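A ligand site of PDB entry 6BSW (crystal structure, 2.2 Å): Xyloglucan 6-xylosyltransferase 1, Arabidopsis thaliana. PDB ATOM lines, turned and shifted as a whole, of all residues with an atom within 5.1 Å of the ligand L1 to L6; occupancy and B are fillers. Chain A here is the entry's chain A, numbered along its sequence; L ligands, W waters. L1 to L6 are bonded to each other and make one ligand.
Water W4 lies within hydrogen-bond range of O1 of LIG L1 (2.7 Å) and NE1 of Trp 139 (2.9 Å). Water W6 bridges the side-chain hydroxyl of Tyr 229 (2.7 Å) and an oxygen (O5) of LG2 L2 (2.7 Å). Water W1 bridges the backbone carbonyl oxygen (O) of Ile 150 (2.7 Å) and an oxygen (O1) of LG3 L3 (2.8 Å). Water W2 lies within hydrogen-bond range of the backbone carbonyl oxygen of His 231 (2.7 Å), an oxygen (O5) of LG2 L2 (2.9 Å) and the backbone NH of Tyr 233 (2.9 Å). Water W5 lies within hydrogen-bond range of O2 of LG3 L3, NE2 of Gln 204 and ND2 of Asn 153.
The backbone carbonyl oxygen (O) of Gly 265 lies within hydrogen-bond range of the backbone NH (N) of Asp 274 (2.7 Å). OE1 of Gln 204 sits close to ND2 of Asn 153 (3.4 Å). The side-chain amide nitrogen (NE2) of Gln 204 sits at hydrogen-bond distance from the backbone carbonyl oxygen (O) of Trp 149, 3.1 Å away. The side-chain hydroxyl (OH) of Tyr 275 lies within hydrogen-bond range of the side-chain hydroxyl (OH) of Tyr 233, at 2.8 Å. ND1 of His 231 sits close to OD1 of Asn 153.
An oxygen (O10) of LG7 L7 sits at hydrogen-bond distance from an oxygen (O5) of LG4 L4 (2.5 Å).
An oxygen (O12) of LG7 L7 sits at hydrogen-bond distance from the backbone NH (N) of Gly 265 (2.9 Å). An oxygen (O1) of LG4 L4 is in hydrogen-bond range of the side-chain hydroxyl (OH) of Tyr 275, 2.9 Å away. The side-chain amino group (NZ) of Lys 267 lies within hydrogen-bond range of an oxygen (O1) of LG5 L5 (3.2 Å). NZ of Lys 267 is in salt-bridge range of O7 of LG7 L7, 2.9 Å away. O1 of LG3 L3 lies within hydrogen-bond range of NE2 of His 231. OD2 of Asp 274 lies within hydrogen-bond range of O5 of LG5 L5, 2.6 Å away. O6 of LIG L1 lies close to SD of Met 142, at 3.7 Å.
Residues that only touch the ligand L1 to L6: Phe 88, Trp 139, Trp 149, Ile 150, Pro 197, Gln 204, Tyr 229, Tyr 233, Val 264 and Gly 265. Hydrophobic or aromatic side chains that line the ligand L1 to L6: Phe 88, Trp 139, Met 142, Trp 149, Ile 150, Pro 197, Tyr 229, His 231, Tyr 233, Val 264 and Tyr 275. Of the 20 residues printed, 15 come within 4 Å of the ligand L1 to L6.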
ATOM      1  N   PHE A  88     -25.141  22.198 -26.174  1.00  0.00           N
ATOM      2  CA  PHE A  88     -24.254  22.815 -25.188  1.00  0.00           C
ATOM      3  C   PHE A  88     -23.989  24.290 -25.486  1.00  0.00           C
ATOM      4  O   PHE A  88     -23.413  24.969 -24.633  1.00  0.00           O
ATOM      5  CB  PHE A  88     -22.919  22.065 -25.082  1.00  0.00           C
ATOM      6  CG  PHE A  88     -22.424  21.489 -26.370  1.00  0.00           C
ATOM      7  CD1 PHE A  88     -22.100  22.305 -27.438  1.00  0.00           C
ATOM      8  CD2 PHE A  88     -22.276  20.117 -26.513  1.00  0.00           C
ATOM      9  CE1 PHE A  88     -21.641  21.769 -28.631  1.00  0.00           C
ATOM     10  CE2 PHE A  88     -21.809  19.575 -27.695  1.00  0.00           C
ATOM     11  CZ  PHE A  88     -21.503  20.402 -28.756  1.00  0.00           C
ATOM     12  N   HIS A 137     -10.988  25.852 -15.014  1.00  0.00           N
ATOM     13  CA  HIS A 137      -9.967  24.860 -14.714  1.00  0.00           C
ATOM     14  C   HIS A 137      -9.172  24.555 -15.976  1.00  0.00           C
ATOM     15  O   HIS A 137      -9.744  24.216 -17.005  1.00  0.00           O
ATOM     16  CB  HIS A 137     -10.595  23.584 -14.163  1.00  0.00           C
ATOM     17  CG  HIS A 137      -9.585  22.575 -13.693  1.00  0.00           C
ATOM     18  ND1 HIS A 137      -9.034  21.625 -14.525  1.00  0.00           N
ATOM     19  CD2 HIS A 137      -9.030  22.367 -12.467  1.00  0.00           C
ATOM     20  CE1 HIS A 137      -8.185  20.879 -13.838  1.00  0.00           C
ATOM     21  NE2 HIS A 137      -8.167  21.314 -12.591  1.00  0.00           N
ATOM     22  N   TRP A 139      -4.773  24.795 -17.809  1.00  0.00           N
ATOM     23  CA  TRP A 139      -3.338  25.060 -17.724  1.00  0.00           C
ATOM     24  C   TRP A 139      -2.943  26.013 -18.845  1.00  0.00           C
ATOM     25  O   TRP A 139      -3.326  25.812 -20.003  1.00  0.00           O
ATOM     26  CB  TRP A 139      -2.530  23.756 -17.831  1.00  0.00           C
ATOM     27  CG  TRP A 139      -2.860  22.765 -16.752  1.00  0.00           C
ATOM     28  CD1 TRP A 139      -2.191  22.595 -15.571  1.00  0.00           C
ATOM     29  CD2 TRP A 139      -3.930  21.816 -16.749  1.00  0.00           C
ATOM     30  NE1 TRP A 139      -2.780  21.589 -14.838  1.00  0.00           N
ATOM     31  CE2 TRP A 139      -3.852  21.103 -15.528  1.00  0.00           C
ATOM     32  CE3 TRP A 139      -4.948  21.500 -17.646  1.00  0.00           C
ATOM     33  CZ2 TRP A 139      -4.751  20.084 -15.199  1.00  0.00           C
ATOM     34  CZ3 TRP A 139      -5.850  20.494 -17.317  1.00  0.00           C
ATOM     35  CH2 TRP A 139      -5.733  19.804 -16.102  1.00  0.00           C
ATOM     36  N   GLU A 141      -0.065  26.478 -20.388  1.00  0.00           N
ATOM     37  CA  GLU A 141       0.738  25.907 -21.465  1.00  0.00           C
ATOM     38  C   GLU A 141      -0.119  25.066 -22.404  1.00  0.00           C
ATOM     39  O   GLU A 141       0.083  25.095 -23.628  1.00  0.00           O
ATOM     40  CB  GLU A 141       1.882  25.077 -20.878  1.00  0.00           C
ATOM     41  CG  GLU A 141       1.474  23.878 -20.018  1.00  0.00           C
ATOM     42  CD  GLU A 141       1.130  24.255 -18.585  1.00  0.00           C
ATOM     43  OE1 GLU A 141       0.944  25.465 -18.314  1.00  0.00           O
ATOM     44  OE2 GLU A 141       1.065  23.350 -17.724  1.00  0.00           O
ATOM     45  N   MET A 142      -1.083  24.309 -21.865  1.00  0.00           N
ATOM     46  CA  MET A 142      -1.896  23.447 -22.707  1.00  0.00           C
ATOM     47  C   MET A 142      -2.862  24.231 -23.581  1.00  0.00           C
ATOM     48  O   MET A 142      -3.269  23.732 -24.637  1.00  0.00           O
ATOM     49  CB  MET A 142      -2.678  22.447 -21.848  1.00  0.00           C
ATOM     50  CG  MET A 142      -1.818  21.314 -21.295  1.00  0.00           C
ATOM     51  SD  MET A 142      -2.803  20.042 -20.479  1.00  0.00           S
ATOM     52  CE  MET A 142      -3.719  19.365 -21.872  1.00  0.00           C
ATOM     53  N   TRP A 149      -7.547  21.014 -27.071  1.00  0.00           N
ATOM     54  CA  TRP A 149      -8.976  21.248 -26.890  1.00  0.00           C
ATOM     55  C   TRP A 149      -9.458  20.874 -25.496  1.00  0.00           C
ATOM     56  O   TRP A 149     -10.601  21.201 -25.147  1.00  0.00           O
ATOM     57  CB  TRP A 149      -9.775  20.473 -27.943  1.00  0.00           C
ATOM     58  CG  TRP A 149      -9.907  19.013 -27.678  1.00  0.00           C
ATOM     59  CD1 TRP A 149      -8.904  18.085 -27.634  1.00  0.00           C
ATOM     60  CD2 TRP A 149     -11.127  18.295 -27.436  1.00  0.00           C
ATOM     61  NE1 TRP A 149      -9.422  16.842 -27.372  1.00  0.00           N
ATOM     62  CE2 TRP A 149     -10.777  16.938 -27.240  1.00  0.00           C
ATOM     63  CE3 TRP A 149     -12.470  18.659 -27.356  1.00  0.00           C
ATOM     64  CZ2 TRP A 149     -11.735  15.960 -26.980  1.00  0.00           C
ATOM     65  CZ3 TRP A 149     -13.415  17.684 -27.094  1.00  0.00           C
ATOM     66  CH2 TRP A 149     -13.039  16.348 -26.905  1.00  0.00           C
ATOM     67  N   ILE A 150      -8.626  20.225 -24.681  1.00  0.00           N
ATOM     68  CA  ILE A 150      -8.954  19.922 -23.298  1.00  0.00           C
ATOM     69  C   ILE A 150      -8.035  20.661 -22.329  1.00  0.00           C
ATOM     70  O   ILE A 150      -7.944  20.311 -21.162  1.00  0.00           O
ATOM     71  CB  ILE A 150      -8.929  18.409 -23.031  1.00  0.00           C
ATOM     72  CG1 ILE A 150      -7.568  17.818 -23.408  1.00  0.00           C
ATOM     73  CG2 ILE A 150     -10.046  17.721 -23.805  1.00  0.00           C
ATOM     74  CD1 ILE A 150      -7.349  16.416 -22.916  1.00  0.00           C
ATOM     75  N   ASN A 153     -11.740  23.678 -19.340  1.00  0.00           N
ATOM     76  CA  ASN A 153     -13.055  23.046 -19.303  1.00  0.00           C
ATOM     77  C   ASN A 153     -14.123  24.102 -19.065  1.00  0.00           C
ATOM     78  O   ASN A 153     -13.996  24.917 -18.152  1.00  0.00           O
ATOM     79  CB  ASN A 153     -13.114  21.978 -18.207  1.00  0.00           C
ATOM     80  CG  ASN A 153     -14.435  21.221 -18.189  1.00  0.00           C
ATOM     81  OD1 ASN A 153     -15.398  21.651 -17.545  1.00  0.00           O
ATOM     82  ND2 ASN A 153     -14.489  20.098 -18.897  1.00  0.00           N
ATOM     83  N   PRO A 197     -11.039  15.344 -31.913  1.00  0.00           N
ATOM     84  CA  PRO A 197     -11.681  14.504 -32.925  1.00  0.00           C
ATOM     85  C   PRO A 197     -12.507  15.337 -33.893  1.00  0.00           C
ATOM     86  O   PRO A 197     -12.521  16.570 -33.811  1.00  0.00           O
ATOM     87  CB  PRO A 197     -12.548  13.549 -32.108  1.00  0.00           C
ATOM     88  CG  PRO A 197     -12.722  14.206 -30.788  1.00  0.00           C
ATOM     89  CD  PRO A 197     -11.473  15.002 -30.543  1.00  0.00           C
ATOM     90  N   PHE A 199     -15.976  16.548 -35.155  1.00  0.00           N
ATOM     91  CA  PHE A 199     -17.398  16.687 -34.860  1.00  0.00           C
ATOM     92  C   PHE A 199     -17.730  18.172 -34.854  1.00  0.00           C
ATOM     93  O   PHE A 199     -16.851  19.036 -34.982  1.00  0.00           O
ATOM     94  CB  PHE A 199     -17.776  16.029 -33.539  1.00  0.00           C
ATOM     95  CG  PHE A 199     -17.132  16.653 -32.323  1.00  0.00           C
ATOM     96  CD1 PHE A 199     -15.777  16.507 -32.091  1.00  0.00           C
ATOM     97  CD2 PHE A 199     -17.894  17.363 -31.414  1.00  0.00           C
ATOM     98  CE1 PHE A 199     -15.184  17.064 -30.982  1.00  0.00           C
ATOM     99  CE2 PHE A 199     -17.311  17.926 -30.296  1.00  0.00           C
ATOM    100  CZ  PHE A 199     -15.954  17.780 -30.074  1.00  0.00           C
ATOM    101  N   GLN A 204     -16.449  24.534 -25.774  1.00  0.00           N
ATOM    102  CA  GLN A 204     -15.137  24.389 -25.145  1.00  0.00           C
ATOM    103  C   GLN A 204     -14.021  24.587 -26.160  1.00  0.00           C
ATOM    104  O   GLN A 204     -13.105  25.380 -25.939  1.00  0.00           O
ATOM    105  CB  GLN A 204     -15.016  23.025 -24.465  1.00  0.00           C
ATOM    106  CG  GLN A 204     -13.662  22.758 -23.838  1.00  0.00           C
ATOM    107  CD  GLN A 204     -13.692  21.620 -22.838  1.00  0.00           C
ATOM    108  OE1 GLN A 204     -14.562  21.573 -21.963  1.00  0.00           O
ATOM    109  NE2 GLN A 204     -12.744  20.703 -22.952  1.00  0.00           N
ATOM    110  N   TYR A 229      -9.882  21.098  -8.093  1.00  0.00           N
ATOM    111  CA  TYR A 229     -10.702  20.564  -9.183  1.00  0.00           C
ATOM    112  C   TYR A 229     -12.020  21.339  -9.287  1.00  0.00           C
ATOM    113  O   TYR A 229     -13.110  20.842  -8.970  1.00  0.00           O
ATOM    114  CB  TYR A 229     -10.951  19.074  -8.983  1.00  0.00           C
ATOM    115  CG  TYR A 229      -9.782  18.206  -9.422  1.00  0.00           C
ATOM    116  CD1 TYR A 229      -9.333  18.227 -10.735  1.00  0.00           C
ATOM    117  CD2 TYR A 229      -9.149  17.356  -8.520  1.00  0.00           C
ATOM    118  CE1 TYR A 229      -8.274  17.437 -11.139  1.00  0.00           C
ATOM    119  CE2 TYR A 229      -8.083  16.561  -8.922  1.00  0.00           C
ATOM    120  CZ  TYR A 229      -7.653  16.607 -10.238  1.00  0.00           C
ATOM    121  OH  TYR A 229      -6.611  15.828 -10.645  1.00  0.00           O
ATOM    122  N   HIS A 231     -13.005  21.787 -12.137  1.00  0.00           N
ATOM    123  CA  HIS A 231     -13.495  20.734 -12.994  1.00  0.00           C
ATOM    124  C   HIS A 231     -12.651  19.490 -12.744  1.00  0.00           C
ATOM    125  O   HIS A 231     -11.414  19.550 -12.864  1.00  0.00           O
ATOM    126  CB  HIS A 231     -13.419  21.108 -14.472  1.00  0.00           C
ATOM    127  CG  HIS A 231     -13.246  19.939 -15.391  1.00  0.00           C
ATOM    128  ND1 HIS A 231     -14.274  19.080 -15.707  1.00  0.00           N
ATOM    129  CD2 HIS A 231     -12.157  19.479 -16.048  1.00  0.00           C
ATOM    130  CE1 HIS A 231     -13.823  18.145 -16.522  1.00  0.00           C
ATOM    131  NE2 HIS A 231     -12.542  18.362 -16.749  1.00  0.00           N
ATOM    132  N   TYR A 233     -12.061  15.654 -13.935  1.00  0.00           N
ATOM    133  CA  TYR A 233     -12.260  14.528 -14.823  1.00  0.00           C
ATOM    134  C   TYR A 233     -12.558  13.264 -14.018  1.00  0.00           C
ATOM    135  O   TYR A 233     -11.705  12.783 -13.263  1.00  0.00           O
ATOM    136  CB  TYR A 233     -11.024  14.322 -15.706  1.00  0.00           C
ATOM    137  CG  TYR A 233     -11.063  13.108 -16.602  1.00  0.00           C
ATOM    138  CD1 TYR A 233     -12.220  12.783 -17.316  1.00  0.00           C
ATOM    139  CD2 TYR A 233      -9.952  12.304 -16.767  1.00  0.00           C
ATOM    140  CE1 TYR A 233     -12.257  11.680 -18.142  1.00  0.00           C
ATOM    141  CE2 TYR A 233      -9.981  11.196 -17.583  1.00  0.00           C
ATOM    142  CZ  TYR A 233     -11.136  10.880 -18.276  1.00  0.00           C
ATOM    143  OH  TYR A 233     -11.159   9.781 -19.101  1.00  0.00           O
ATOM    144  N   ILE A 236     -10.197   9.831 -13.497  1.00  0.00           N
ATOM    145  CA  ILE A 236      -9.042   9.698 -12.636  1.00  0.00           C
ATOM    146  C   ILE A 236      -9.384   9.953 -11.172  1.00  0.00           C
ATOM    147  O   ILE A 236      -8.480  10.060 -10.327  1.00  0.00           O
ATOM    148  CB  ILE A 236      -7.896  10.629 -13.083  1.00  0.00           C
ATOM    149  CG1 ILE A 236      -8.351  12.095 -13.052  1.00  0.00           C
ATOM    150  CG2 ILE A 236      -7.431  10.245 -14.479  1.00  0.00           C
ATOM    151  CD1 ILE A 236      -7.229  13.084 -13.241  1.00  0.00           C
ATOM    152  N   VAL A 264     -17.703  13.909 -17.884  1.00  0.00           N
ATOM    153  CA  VAL A 264     -17.550  14.230 -19.301  1.00  0.00           C
ATOM    154  C   VAL A 264     -17.518  12.954 -20.126  1.00  0.00           C
ATOM    155  O   VAL A 264     -16.893  11.957 -19.747  1.00  0.00           O
ATOM    156  CB  VAL A 264     -16.280  15.068 -19.518  1.00  0.00           C
ATOM    157  CG1 VAL A 264     -16.392  16.415 -18.825  1.00  0.00           C
ATOM    158  CG2 VAL A 264     -15.045  14.306 -19.021  1.00  0.00           C
ATOM    159  N   GLY A 265     -18.195  12.986 -21.275  1.00  0.00           N
ATOM    160  CA  GLY A 265     -18.203  11.871 -22.189  1.00  0.00           C
ATOM    161  C   GLY A 265     -19.215  10.782 -21.884  1.00  0.00           C
ATOM    162  O   GLY A 265     -19.346   9.855 -22.686  1.00  0.00           O
ATOM    163  N   LYS A 267     -22.778  11.149 -21.038  1.00  0.00           N
ATOM    164  CA  LYS A 267     -24.093  11.353 -21.629  1.00  0.00           C
ATOM    165  C   LYS A 267     -25.139  10.506 -20.918  1.00  0.00           C
ATOM    166  O   LYS A 267     -25.803   9.678 -21.559  1.00  0.00           O
ATOM    167  CB  LYS A 267     -24.081  11.023 -23.125  1.00  0.00           C
ATOM    168  CG  LYS A 267     -23.009  11.742 -23.922  1.00  0.00           C
ATOM    169  CD  LYS A 267     -23.035  13.241 -23.654  1.00  0.00           C
ATOM    170  CE  LYS A 267     -22.002  13.987 -24.476  1.00  0.00           C
ATOM    171  NZ  LYS A 267     -21.726  15.334 -23.903  1.00  0.00           N
ATOM    172  N   ASP A 274     -18.810   8.380 -24.854  1.00  0.00           N
ATOM    173  CA  ASP A 274     -17.479   7.832 -25.084  1.00  0.00           C
ATOM    174  C   ASP A 274     -17.121   6.691 -24.143  1.00  0.00           C
ATOM    175  O   ASP A 274     -16.075   6.060 -24.329  1.00  0.00           O
ATOM    176  CB  ASP A 274     -16.423   8.936 -24.960  1.00  0.00           C
ATOM    177  CG  ASP A 274     -16.365   9.846 -26.175  1.00  0.00           C
ATOM    178  OD1 ASP A 274     -17.140   9.618 -27.132  1.00  0.00           O
ATOM    179  OD2 ASP A 274     -15.541  10.783 -26.170  1.00  0.00           O
ATOM    180  N   TYR A 275     -17.952   6.411 -23.150  1.00  0.00           N
ATOM    181  CA  TYR A 275     -17.689   5.352 -22.182  1.00  0.00           C
ATOM    182  C   TYR A 275     -18.945   4.507 -22.004  1.00  0.00           C
ATOM    183  O   TYR A 275     -20.051   4.951 -22.317  1.00  0.00           O
ATOM    184  CB  TYR A 275     -17.258   5.934 -20.832  1.00  0.00           C
ATOM    185  CG  TYR A 275     -16.137   6.940 -20.930  1.00  0.00           C
ATOM    186  CD1 TYR A 275     -14.811   6.537 -20.981  1.00  0.00           C
ATOM    187  CD2 TYR A 275     -16.405   8.307 -20.984  1.00  0.00           C
ATOM    188  CE1 TYR A 275     -13.781   7.459 -21.070  1.00  0.00           C
ATOM    189  CE2 TYR A 275     -15.384   9.233 -21.074  1.00  0.00           C
ATOM    190  CZ  TYR A 275     -14.075   8.805 -21.117  1.00  0.00           C
ATOM    191  OH  TYR A 275     -13.062   9.737 -21.208  1.00  0.00           O
HETATM  192  C1  LIG L   1      -1.564  16.766 -13.411  1.00  0.00           C
HETATM  193  C2  LIG L   1      -2.079  15.937 -14.526  1.00  0.00           C
HETATM  194  C3  LIG L   1      -2.415  16.752 -15.742  1.00  0.00           C
HETATM  195  C4  LIG L   1      -1.242  17.618 -16.164  1.00  0.00           C
HETATM  196  C5  LIG L   1      -1.634  18.488 -17.328  1.00  0.00           C
HETATM  197  C6  LIG L   1      -0.431  17.682 -13.838  1.00  0.00           C
HETATM  198  O1  LIG L   1      -0.141  18.530 -12.823  1.00  0.00           O
HETATM  199  O2  LIG L   1      -1.076  15.891 -12.355  1.00  0.00           O
HETATM  200  O3  LIG L   1      -3.266  15.243 -14.068  1.00  0.00           O
HETATM  201  O4  LIG L   1      -2.759  15.860 -16.824  1.00  0.00           O
HETATM  202  O5  LIG L   1      -0.794  18.491 -15.058  1.00  0.00           O
HETATM  203  O6  LIG L   1      -0.668  19.479 -17.506  1.00  0.00           O
HETATM  204  C1  LG2 L   2      -4.132  15.457 -18.725  1.00  0.00           C
HETATM  205  C2  LG2 L   2      -5.455  15.716 -19.358  1.00  0.00           C
HETATM  206  C3  LG2 L   2      -6.623  15.604 -18.431  1.00  0.00           C
HETATM  207  C4  LG2 L   2      -6.377  16.291 -17.076  1.00  0.00           C
HETATM  208  C5  LG2 L   2      -7.489  15.940 -16.109  1.00  0.00           C
HETATM  209  C6  LG2 L   2      -3.964  16.219 -17.412  1.00  0.00           C
HETATM  210  O1  LG2 L   2      -3.111  15.885 -19.635  1.00  0.00           O
HETATM  211  O2  LG2 L   2      -5.652  14.755 -20.440  1.00  0.00           O
HETATM  212  O3  LG2 L   2      -7.747  16.247 -19.073  1.00  0.00           O
HETATM  213  O4  LG2 L   2      -5.089  15.914 -16.477  1.00  0.00           O
HETATM  214  O5  LG2 L   2      -7.388  16.766 -14.957  1.00  0.00           O
HETATM  215  C1  LG3 L   3     -10.039  16.307 -19.487  1.00  0.00           C
HETATM  216  C2  LG3 L   3     -11.268  15.544 -19.891  1.00  0.00           C
HETATM  217  C3  LG3 L   3     -10.981  14.526 -20.939  1.00  0.00           C
HETATM  218  C4  LG3 L   3      -9.854  13.600 -20.495  1.00  0.00           C
HETATM  219  C5  LG3 L   3      -9.568  12.559 -21.552  1.00  0.00           C
HETATM  220  C6  LG3 L   3      -8.854  15.424 -19.177  1.00  0.00           C
HETATM  221  O1  LG3 L   3     -10.329  17.069 -18.305  1.00  0.00           O
HETATM  222  O2  LG3 L   3     -12.244  16.487 -20.396  1.00  0.00           O
HETATM  223  O3  LG3 L   3     -12.200  13.736 -21.200  1.00  0.00           O
HETATM  224  O4  LG3 L   3      -8.619  14.379 -20.231  1.00  0.00           O
HETATM  225  O5  LG3 L   3      -9.417  13.177 -22.802  1.00  0.00           O
HETATM  226  C1  LG4 L   4     -13.894  13.218 -22.788  1.00  0.00           C
HETATM  227  C2  LG4 L   4     -14.703  13.676 -23.961  1.00  0.00           C
HETATM  228  C3  LG4 L   4     -15.311  15.000 -23.737  1.00  0.00           C
HETATM  229  C4  LG4 L   4     -14.224  16.042 -23.355  1.00  0.00           C
HETATM  230  C5  LG4 L   4     -14.803  17.296 -23.066  1.00  0.00           C
HETATM  231  C6  LG4 L   4     -12.860  14.197 -22.393  1.00  0.00           C
HETATM  232  O1  LG4 L   4     -13.251  11.939 -23.130  1.00  0.00           O
HETATM  233  O2  LG4 L   4     -15.713  12.622 -24.181  1.00  0.00           O
HETATM  234  O3  LG4 L   4     -15.985  15.575 -24.913  1.00  0.00           O
HETATM  235  O4  LG4 L   4     -13.450  15.506 -22.116  1.00  0.00           O
HETATM  236  O5  LG4 L   4     -15.846  17.149 -22.092  1.00  0.00           O
HETATM  237  C1  LG5 L   5     -17.927  15.491 -26.258  1.00  0.00           C
HETATM  238  C2  LG5 L   5     -18.730  14.726 -27.241  1.00  0.00           C
HETATM  239  C3  LG5 L   5     -17.925  14.069 -28.296  1.00  0.00           C
HETATM  240  C4  LG5 L   5     -16.713  13.247 -27.731  1.00  0.00           C
HETATM  241  C5  LG5 L   5     -15.834  12.874 -28.790  1.00  0.00           C
HETATM  242  C6  LG5 L   5     -16.799  14.708 -25.685  1.00  0.00           C
HETATM  243  O1  LG5 L   5     -18.822  15.882 -25.171  1.00  0.00           O
HETATM  244  O2  LG5 L   5     -19.681  15.675 -27.895  1.00  0.00           O
HETATM  245  O3  LG5 L   5     -18.766  13.155 -29.000  1.00  0.00           O
HETATM  246  O4  LG5 L   5     -15.939  14.122 -26.723  1.00  0.00           O
HETATM  247  O5  LG5 L   5     -14.692  12.203 -28.237  1.00  0.00           O
HETATM  248  C1  LG6 L   6     -19.550  12.469 -31.112  1.00  0.00           C
HETATM  249  C2  LG6 L   6     -20.309  12.841 -32.347  1.00  0.00           C
HETATM  250  C3  LG6 L   6     -21.547  13.595 -32.016  1.00  0.00           C
HETATM  251  C4  LG6 L   6     -21.255  14.807 -31.157  1.00  0.00           C
HETATM  252  C5  LG6 L   6     -22.556  15.454 -30.773  1.00  0.00           C
HETATM  253  C6  LG6 L   6     -19.279  13.656 -30.214  1.00  0.00           C
HETATM  254  O1  LG6 L   6     -18.295  11.898 -31.503  1.00  0.00           O
HETATM  255  O2  LG6 L   6     -20.672  11.628 -33.054  1.00  0.00           O
HETATM  256  O3  LG6 L   6     -22.160  14.029 -33.243  1.00  0.00           O
HETATM  257  O4  LG6 L   6     -20.499  14.448 -29.923  1.00  0.00           O
HETATM  258  O5  LG6 L   6     -22.353  16.329 -29.699  1.00  0.00           O
HETATM  259  N1  LG7 L   7     -27.280  21.395 -21.825  1.00  0.00           N
HETATM  260  C1  LG7 L   7     -28.458  22.291 -21.872  1.00  0.00           C
HETATM  261  N2  LG7 L   7     -29.527  22.052 -22.908  1.00  0.00           N
HETATM  262  C2  LG7 L   7     -29.419  20.962 -23.857  1.00  0.00           C
HETATM  263  C3  LG7 L   7     -28.219  20.064 -23.807  1.00  0.00           C
HETATM  264  C4  LG7 L   7     -27.171  20.305 -22.785  1.00  0.00           C
HETATM  265  O1  LG7 L   7     -28.566  23.170 -21.112  1.00  0.00           O
HETATM  266  O2  LG7 L   7     -30.280  20.800 -24.665  1.00  0.00           O
HETATM  267  C5  LG7 L   7     -26.345  21.621 -20.918  1.00  0.00           C
HETATM  268  C6  LG7 L   7     -26.239  20.478 -19.890  1.00  0.00           C
HETATM  269  O3  LG7 L   7     -25.983  21.042 -18.562  1.00  0.00           O
HETATM  270  C7  LG7 L   7     -25.190  19.766 -20.296  1.00  0.00           C
HETATM  271  C8  LG7 L   7     -24.174  20.854 -20.974  1.00  0.00           C
HETATM  272  O4  LG7 L   7     -24.942  21.700 -21.622  1.00  0.00           O
HETATM  273  O5  LG7 L   7     -24.535  19.125 -19.202  1.00  0.00           O
HETATM  274  C9  LG7 L   7     -23.252  20.163 -21.912  1.00  0.00           C
HETATM  275  O6  LG7 L   7     -22.391  19.358 -21.161  1.00  0.00           O
HETATM  276  P1  LG7 L   7     -22.138  17.773 -21.560  1.00  0.00           P
HETATM  277  O7  LG7 L   7     -23.263  17.211 -22.387  1.00  0.00           O
HETATM  278  O8  LG7 L   7     -22.018  16.993 -20.262  1.00  0.00           O
HETATM  279  O9  LG7 L   7     -20.736  17.649 -22.412  1.00  0.00           O
HETATM  280  P2  LG7 L   7     -19.449  16.824 -21.807  1.00  0.00           P
HETATM  281  O10 LG7 L   7     -18.270  16.965 -22.753  1.00  0.00           O
HETATM  282  O11 LG7 L   7     -19.128  17.440 -20.452  1.00  0.00           O
HETATM  283  O12 LG7 L   7     -19.841  15.358 -21.667  1.00  0.00           O
HETATM  284  O   HOH W   1      -9.590  19.642 -19.121  1.00  0.00           O
HETATM  285  O   HOH W   2      -9.967  17.687 -14.100  1.00  0.00           O
HETATM  286  O   HOH W   3      -3.152  15.424 -22.530  1.00  0.00           O
HETATM  287  O   HOH W   4      -2.104  20.327 -12.290  1.00  0.00           O
HETATM  288  O   HOH W   5     -11.934  19.360 -20.456  1.00  0.00           O
HETATM  289  O   HOH W   6      -5.500  16.466 -13.019  1.00  0.00           O
HETATM  290  O   HOH W   7      -4.236  13.105 -15.741  1.00  0.00           O
